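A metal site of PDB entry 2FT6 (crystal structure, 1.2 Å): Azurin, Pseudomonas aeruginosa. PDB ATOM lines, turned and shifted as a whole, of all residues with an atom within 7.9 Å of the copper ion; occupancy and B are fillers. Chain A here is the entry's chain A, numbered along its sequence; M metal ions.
O of Asn 10 sits at hydrogen-bond distance from NE2 of His 46, 2.7 Å away. The backbone carbonyl oxygen (O) of His 46 sits at hydrogen-bond distance from the backbone NH (N) of Ile 87, at 2.8 Å. ND1 of His 46 sits close to SD of Met 117 (3.5 Å). SG of Cys 112 lies close to N of Asn 47 (3.5 Å). The backbone NH (N) of Cys 112 sits at hydrogen-bond distance from the backbone carbonyl oxygen (O) of Met 117, at 3.2 Å.
O of Gly 45 touches the copper ion, at 3.3 Å. SD of Met 117 touches the copper ion (3.1 Å). Of the 22 residues printed, 5 come within 4 Å of the copper ion. The nearest printed residue that does not touch the copper ion is Pro 114 (4.1 Å).
The copper ion is bound by ND1 of His 115 (2.0 Å), ND1 of His 46 (2.1 Å) and SG of Cys 112 (2.1 Å).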
ATOM      1  N   GLY A   9      -6.245 -26.243  -6.424  1.00  0.00           N
ATOM      2  CA  GLY A   9      -6.072 -24.804  -6.305  1.00  0.00           C
ATOM      3  C   GLY A   9      -4.913 -24.569  -5.366  1.00  0.00           C
ATOM      4  O   GLY A   9      -4.841 -25.158  -4.298  1.00  0.00           O
ATOM      5  N   ASN A  10      -3.994 -23.685  -5.746  1.00  0.00           N
ATOM      6  CA  ASN A  10      -2.699 -23.516  -5.037  1.00  0.00           C
ATOM      7  C   ASN A  10      -2.616 -22.166  -4.318  1.00  0.00           C
ATOM      8  O   ASN A  10      -3.591 -21.419  -4.231  1.00  0.00           O
ATOM      9  CB  ASN A  10      -1.556 -23.784  -5.982  1.00  0.00           C
ATOM     10  CG  ASN A  10      -1.391 -22.700  -7.054  1.00  0.00           C
ATOM     11  OD1 ASN A  10      -2.022 -21.653  -6.993  1.00  0.00           O
ATOM     12  ND2 ASN A  10      -0.512 -22.957  -8.046  1.00  0.00           N
ATOM     13  N   MET A  13      -3.465 -18.736  -6.215  1.00  0.00           N
ATOM     14  CA  MET A  13      -4.813 -18.506  -6.743  1.00  0.00           C
ATOM     15  C   MET A  13      -4.931 -19.016  -8.176  1.00  0.00           C
ATOM     16  O   MET A  13      -5.493 -18.357  -9.024  1.00  0.00           O
ATOM     17  CB  MET A  13      -5.289 -17.063  -6.709  1.00  0.00           C
ATOM     18  CG  MET A  13      -5.341 -16.420  -5.414  1.00  0.00           C
ATOM     19  SD  MET A  13      -5.876 -14.681  -5.545  1.00  0.00           S
ATOM     20  CE  MET A  13      -4.589 -13.970  -6.602  1.00  0.00           C
ATOM     21  N   GLN A  14      -4.406 -20.201  -8.408  1.00  0.00           N
ATOM     22  CA  GLN A  14      -4.498 -20.858  -9.699  1.00  0.00           C
ATOM     23  C   GLN A  14      -5.150 -22.215  -9.552  1.00  0.00           C
ATOM     24  O   GLN A  14      -4.734 -23.009  -8.733  1.00  0.00           O
ATOM     25  CB  GLN A  14      -3.113 -21.122 -10.286  1.00  0.00           C
ATOM     26  CG  GLN A  14      -2.345 -19.835 -10.564  1.00  0.00           C
ATOM     27  CD  GLN A  14      -0.856 -20.034 -10.758  1.00  0.00           C
ATOM     28  OE1 GLN A  14      -0.253 -21.002 -10.318  1.00  0.00           O
ATOM     29  NE2 GLN A  14      -0.240 -19.022 -11.383  1.00  0.00           N
ATOM     30  N   PHE A  15      -6.148 -22.473 -10.389  1.00  0.00           N
ATOM     31  CA  PHE A  15      -6.587 -23.863 -10.619  1.00  0.00           C
ATOM     32  C   PHE A  15      -5.635 -24.503 -11.609  1.00  0.00           C
ATOM     33  O   PHE A  15      -5.079 -23.820 -12.472  1.00  0.00           O
ATOM     34  CB  PHE A  15      -8.015 -23.917 -11.201  1.00  0.00           C
ATOM     35  CG  PHE A  15      -9.144 -23.665 -10.248  1.00  0.00           C
ATOM     36  CD1 PHE A  15      -9.316 -24.414  -9.124  1.00  0.00           C
ATOM     37  CD2 PHE A  15     -10.131 -22.763 -10.580  1.00  0.00           C
ATOM     38  CE1 PHE A  15     -10.415 -24.267  -8.291  1.00  0.00           C
ATOM     39  CE2 PHE A  15     -11.252 -22.594  -9.753  1.00  0.00           C
ATOM     40  CZ  PHE A  15     -11.395 -23.337  -8.628  1.00  0.00           C
ATOM     41  N   LEU A  33     -11.426 -31.905  -5.318  1.00  0.00           N
ATOM     42  CA  LEU A  33     -10.617 -30.680  -5.152  1.00  0.00           C
ATOM     43  C   LEU A  33      -9.594 -30.928  -4.062  1.00  0.00           C
ATOM     44  O   LEU A  33      -9.874 -31.443  -3.000  1.00  0.00           O
ATOM     45  CB  LEU A  33     -11.556 -29.541  -4.738  1.00  0.00           C
ATOM     46  CG  LEU A  33     -10.905 -28.175  -4.582  1.00  0.00           C
ATOM     47  CD1 LEU A  33     -10.404 -27.639  -5.893  1.00  0.00           C
ATOM     48  CD2 LEU A  33     -11.853 -27.173  -3.915  1.00  0.00           C
ATOM     49  N   HIS A  35      -5.599 -28.916  -2.517  1.00  0.00           N
ATOM     50  CA  HIS A  35      -4.923 -27.601  -2.357  1.00  0.00           C
ATOM     51  C   HIS A  35      -3.476 -27.784  -1.960  1.00  0.00           C
ATOM     52  O   HIS A  35      -3.100 -27.670  -0.792  1.00  0.00           O
ATOM     53  CB  HIS A  35      -5.705 -26.829  -1.284  1.00  0.00           C
ATOM     54  CG  HIS A  35      -5.314 -25.365  -1.102  1.00  0.00           C
ATOM     55  ND1 HIS A  35      -4.029 -24.864  -1.273  1.00  0.00           N
ATOM     56  CD2 HIS A  35      -6.053 -24.347  -0.629  1.00  0.00           C
ATOM     57  CE1 HIS A  35      -4.024 -23.560  -0.940  1.00  0.00           C
ATOM     58  NE2 HIS A  35      -5.245 -23.239  -0.540  1.00  0.00           N
ATOM     59  N   MET A  44      -6.175 -18.356   2.245  1.00  0.00           N
ATOM     60  CA  MET A  44      -6.055 -18.845   0.881  1.00  0.00           C
ATOM     61  C   MET A  44      -6.972 -20.051   0.736  1.00  0.00           C
ATOM     62  O   MET A  44      -6.599 -21.060   0.169  1.00  0.00           O
ATOM     63  CB  MET A  44      -4.614 -19.171   0.540  1.00  0.00           C
ATOM     64  CG  MET A  44      -4.337 -19.395  -0.911  1.00  0.00           C
ATOM     65  SD  MET A  44      -4.867 -18.110  -2.068  1.00  0.00           S
ATOM     66  CE  MET A  44      -3.816 -16.707  -1.554  1.00  0.00           C
ATOM     67  N   GLY A  45      -8.197 -19.929   1.167  1.00  0.00           N
ATOM     68  CA  GLY A  45      -9.215 -20.943   0.952  1.00  0.00           C
ATOM     69  C   GLY A  45      -9.755 -20.942  -0.446  1.00  0.00           C
ATOM     70  O   GLY A  45     -10.025 -19.910  -0.977  1.00  0.00           O
ATOM     71  N   HIS A  46      -9.964 -22.173  -0.974  1.00  0.00           N
ATOM     72  CA  HIS A  46     -10.586 -22.312  -2.287  1.00  0.00           C
ATOM     73  C   HIS A  46     -11.823 -23.191  -2.191  1.00  0.00           C
ATOM     74  O   HIS A  46     -11.840 -24.144  -1.438  1.00  0.00           O
ATOM     75  CB  HIS A  46      -9.660 -22.972  -3.285  1.00  0.00           C
ATOM     76  CG  HIS A  46      -8.365 -22.244  -3.506  1.00  0.00           C
ATOM     77  ND1 HIS A  46      -8.310 -20.905  -3.816  1.00  0.00           N
ATOM     78  CD2 HIS A  46      -7.085 -22.688  -3.477  1.00  0.00           C
ATOM     79  CE1 HIS A  46      -7.036 -20.547  -3.927  1.00  0.00           C
ATOM     80  NE2 HIS A  46      -6.267 -21.606  -3.769  1.00  0.00           N
ATOM     81  N   ASN A  47     -12.783 -22.873  -3.041  1.00  0.00           N
ATOM     82  CA  ASN A  47     -13.904 -23.802  -3.302  1.00  0.00           C
ATOM     83  C   ASN A  47     -13.951 -24.013  -4.819  1.00  0.00           C
ATOM     84  O   ASN A  47     -13.259 -23.420  -5.604  1.00  0.00           O
ATOM     85  CB  ASN A  47     -15.203 -23.299  -2.649  1.00  0.00           C
ATOM     86  CG  ASN A  47     -15.635 -21.915  -3.062  1.00  0.00           C
ATOM     87  OD1 ASN A  47     -15.268 -21.450  -4.123  1.00  0.00           O
ATOM     88  ND2 ASN A  47     -16.400 -21.205  -2.221  1.00  0.00           N
ATOM     89  N   TRP A  48     -14.854 -24.957  -5.171  1.00  0.00           N
ATOM     90  CA  TRP A  48     -15.160 -25.249  -6.570  1.00  0.00           C
ATOM     91  C   TRP A  48     -16.661 -25.220  -6.654  1.00  0.00           C
ATOM     92  O   TRP A  48     -17.352 -25.975  -5.982  1.00  0.00           O
ATOM     93  CB  TRP A  48     -14.554 -26.600  -6.986  1.00  0.00           C
ATOM     94  CG  TRP A  48     -14.764 -26.943  -8.429  1.00  0.00           C
ATOM     95  CD1 TRP A  48     -13.879 -26.739  -9.425  1.00  0.00           C
ATOM     96  CD2 TRP A  48     -15.939 -27.521  -9.074  1.00  0.00           C
ATOM     97  NE1 TRP A  48     -14.392 -27.148 -10.636  1.00  0.00           N
ATOM     98  CE2 TRP A  48     -15.657 -27.622 -10.443  1.00  0.00           C
ATOM     99  CE3 TRP A  48     -17.149 -27.972  -8.611  1.00  0.00           C
ATOM    100  CZ2 TRP A  48     -16.592 -28.133 -11.376  1.00  0.00           C
ATOM    101  CZ3 TRP A  48     -18.080 -28.476  -9.539  1.00  0.00           C
ATOM    102  CH2 TRP A  48     -17.777 -28.550 -10.886  1.00  0.00           C
ATOM    103  N   TYR A  72     -18.012 -19.011   1.856  1.00  0.00           N
ATOM    104  CA  TYR A  72     -18.194 -17.957   0.866  1.00  0.00           C
ATOM    105  C   TYR A  72     -19.247 -18.312  -0.187  1.00  0.00           C
ATOM    106  O   TYR A  72     -19.113 -18.012  -1.382  1.00  0.00           O
ATOM    107  CB  TYR A  72     -16.897 -17.560   0.224  1.00  0.00           C
ATOM    108  CG  TYR A  72     -15.893 -16.918   1.169  1.00  0.00           C
ATOM    109  CD1 TYR A  72     -16.218 -15.741   1.798  1.00  0.00           C
ATOM    110  CD2 TYR A  72     -14.642 -17.448   1.331  1.00  0.00           C
ATOM    111  CE1 TYR A  72     -15.283 -15.106   2.669  1.00  0.00           C
ATOM    112  CE2 TYR A  72     -13.696 -16.831   2.196  1.00  0.00           C
ATOM    113  CZ  TYR A  72     -14.065 -15.681   2.807  1.00  0.00           C
ATOM    114  OH  TYR A  72     -13.120 -15.061   3.613  1.00  0.00           O
ATOM    115  N   LEU A  86     -15.143 -24.878   1.312  1.00  0.00           N
ATOM    116  CA  LEU A  86     -13.898 -24.161   1.223  1.00  0.00           C
ATOM    117  C   LEU A  86     -12.781 -24.975   1.898  1.00  0.00           C
ATOM    118  O   LEU A  86     -12.973 -25.439   3.018  1.00  0.00           O
ATOM    119  CB  LEU A  86     -14.032 -22.788   1.930  1.00  0.00           C
ATOM    120  CG  LEU A  86     -12.988 -21.730   1.606  1.00  0.00           C
ATOM    121  CD1 LEU A  86     -13.301 -21.115   0.268  1.00  0.00           C
ATOM    122  CD2 LEU A  86     -12.992 -20.673   2.693  1.00  0.00           C
ATOM    123  N   ILE A  87     -11.637 -25.105   1.221  1.00  0.00           N
ATOM    124  CA  ILE A  87     -10.514 -25.862   1.727  1.00  0.00           C
ATOM    125  C   ILE A  87      -9.240 -25.047   1.786  1.00  0.00           C
ATOM    126  O   ILE A  87      -8.971 -24.215   0.931  1.00  0.00           O
ATOM    127  CB  ILE A  87     -10.282 -27.193   0.933  1.00  0.00           C
ATOM    128  CG1 ILE A  87      -9.874 -26.953  -0.514  1.00  0.00           C
ATOM    129  CG2 ILE A  87     -11.496 -28.108   1.017  1.00  0.00           C
ATOM    130  CD1 ILE A  87      -9.347 -28.185  -1.225  1.00  0.00           C
ATOM    131  N   PHE A 111     -15.808 -22.091 -10.709  1.00  0.00           N
ATOM    132  CA  PHE A 111     -15.077 -20.958 -10.119  1.00  0.00           C
ATOM    133  C   PHE A 111     -14.916 -21.173  -8.658  1.00  0.00           C
ATOM    134  O   PHE A 111     -15.640 -21.939  -8.015  1.00  0.00           O
ATOM    135  CB  PHE A 111     -15.778 -19.613 -10.454  1.00  0.00           C
ATOM    136  CG  PHE A 111     -17.254 -19.627 -10.195  1.00  0.00           C
ATOM    137  CD1 PHE A 111     -18.174 -20.078 -11.161  1.00  0.00           C
ATOM    138  CD2 PHE A 111     -17.764 -19.158  -8.997  1.00  0.00           C
ATOM    139  CE1 PHE A 111     -19.509 -20.113 -10.950  1.00  0.00           C
ATOM    140  CE2 PHE A 111     -19.128 -19.200  -8.787  1.00  0.00           C
ATOM    141  CZ  PHE A 111     -19.994 -19.676  -9.773  1.00  0.00           C
ATOM    142  N   CYS A 112     -13.940 -20.419  -8.101  1.00  0.00           N
ATOM    143  CA  CYS A 112     -13.766 -20.247  -6.670  1.00  0.00           C
ATOM    144  C   CYS A 112     -14.402 -18.898  -6.336  1.00  0.00           C
ATOM    145  O   CYS A 112     -14.102 -17.915  -7.001  1.00  0.00           O
ATOM    146  CB  CYS A 112     -12.262 -20.238  -6.361  1.00  0.00           C
ATOM    147  SG  CYS A 112     -11.947 -19.855  -4.623  1.00  0.00           S
ATOM    148  N   THR A 113     -15.242 -18.831  -5.329  1.00  0.00           N
ATOM    149  CA  THR A 113     -15.895 -17.534  -5.078  1.00  0.00           C
ATOM    150  C   THR A 113     -14.992 -16.414  -4.521  1.00  0.00           C
ATOM    151  O   THR A 113     -15.160 -15.279  -4.960  1.00  0.00           O
ATOM    152  CB  THR A 113     -17.202 -17.713  -4.294  1.00  0.00           C
ATOM    153  OG1 THR A 113     -16.971 -18.370  -3.031  1.00  0.00           O
ATOM    154  CG2 THR A 113     -18.300 -18.394  -5.102  1.00  0.00           C
ATOM    155  N   PRO A 114     -14.087 -16.682  -3.554  1.00  0.00           N
ATOM    156  CA  PRO A 114     -13.257 -15.519  -3.093  1.00  0.00           C
ATOM    157  C   PRO A 114     -12.194 -15.032  -4.015  1.00  0.00           C
ATOM    158  O   PRO A 114     -11.639 -13.950  -3.751  1.00  0.00           O
ATOM    159  CB  PRO A 114     -12.678 -16.050  -1.774  1.00  0.00           C
ATOM    160  CG  PRO A 114     -12.613 -17.563  -1.950  1.00  0.00           C
ATOM    161  CD  PRO A 114     -13.944 -17.818  -2.647  1.00  0.00           C
ATOM    162  N   HIS A 115     -11.818 -15.791  -5.062  1.00  0.00           N
ATOM    163  CA  HIS A 115     -10.665 -15.447  -5.855  1.00  0.00           C
ATOM    164  C   HIS A 115     -10.989 -15.344  -7.302  1.00  0.00           C
ATOM    165  O   HIS A 115     -11.977 -15.963  -7.776  1.00  0.00           O
ATOM    166  CB  HIS A 115      -9.570 -16.495  -5.699  1.00  0.00           C
ATOM    167  CG  HIS A 115      -9.061 -16.610  -4.315  1.00  0.00           C
ATOM    168  ND1 HIS A 115      -9.038 -17.815  -3.618  1.00  0.00           N
ATOM    169  CD2 HIS A 115      -8.590 -15.656  -3.483  1.00  0.00           C
ATOM    170  CE1 HIS A 115      -8.549 -17.577  -2.414  1.00  0.00           C
ATOM    171  NE2 HIS A 115      -8.276 -16.275  -2.290  1.00  0.00           N
ATOM    172  N   PRO A 116     -10.136 -14.681  -8.065  1.00  0.00           N
ATOM    173  CA  PRO A 116     -10.286 -14.608  -9.507  1.00  0.00           C
ATOM    174  C   PRO A 116      -9.794 -15.873 -10.200  1.00  0.00           C
ATOM    175  O   PRO A 116      -8.733 -15.917 -10.833  1.00  0.00           O
ATOM    176  CB  PRO A 116      -9.415 -13.344  -9.834  1.00  0.00           C
ATOM    177  CG  PRO A 116      -8.337 -13.401  -8.847  1.00  0.00           C
ATOM    178  CD  PRO A 116      -9.055 -13.772  -7.577  1.00  0.00           C
ATOM    179  N   MET A 117     -10.569 -16.937 -10.026  1.00  0.00           N
ATOM    180  CA  MET A 117     -10.223 -18.286 -10.517  1.00  0.00           C
ATOM    181  C   MET A 117     -11.470 -18.878 -11.171  1.00  0.00           C
ATOM    182  O   MET A 117     -12.480 -18.992 -10.501  1.00  0.00           O
ATOM    183  CB  MET A 117      -9.861 -19.185  -9.333  1.00  0.00           C
ATOM    184  CG  MET A 117      -8.570 -18.827  -8.688  1.00  0.00           C
ATOM    185  SD  MET A 117      -8.363 -19.549  -7.028  1.00  0.00           S
ATOM    186  CE  MET A 117      -8.292 -21.300  -7.393  1.00  0.00           C
HETATM  187 CU    CU M   1      -9.847 -19.576  -4.261  1.00  0.00          CU
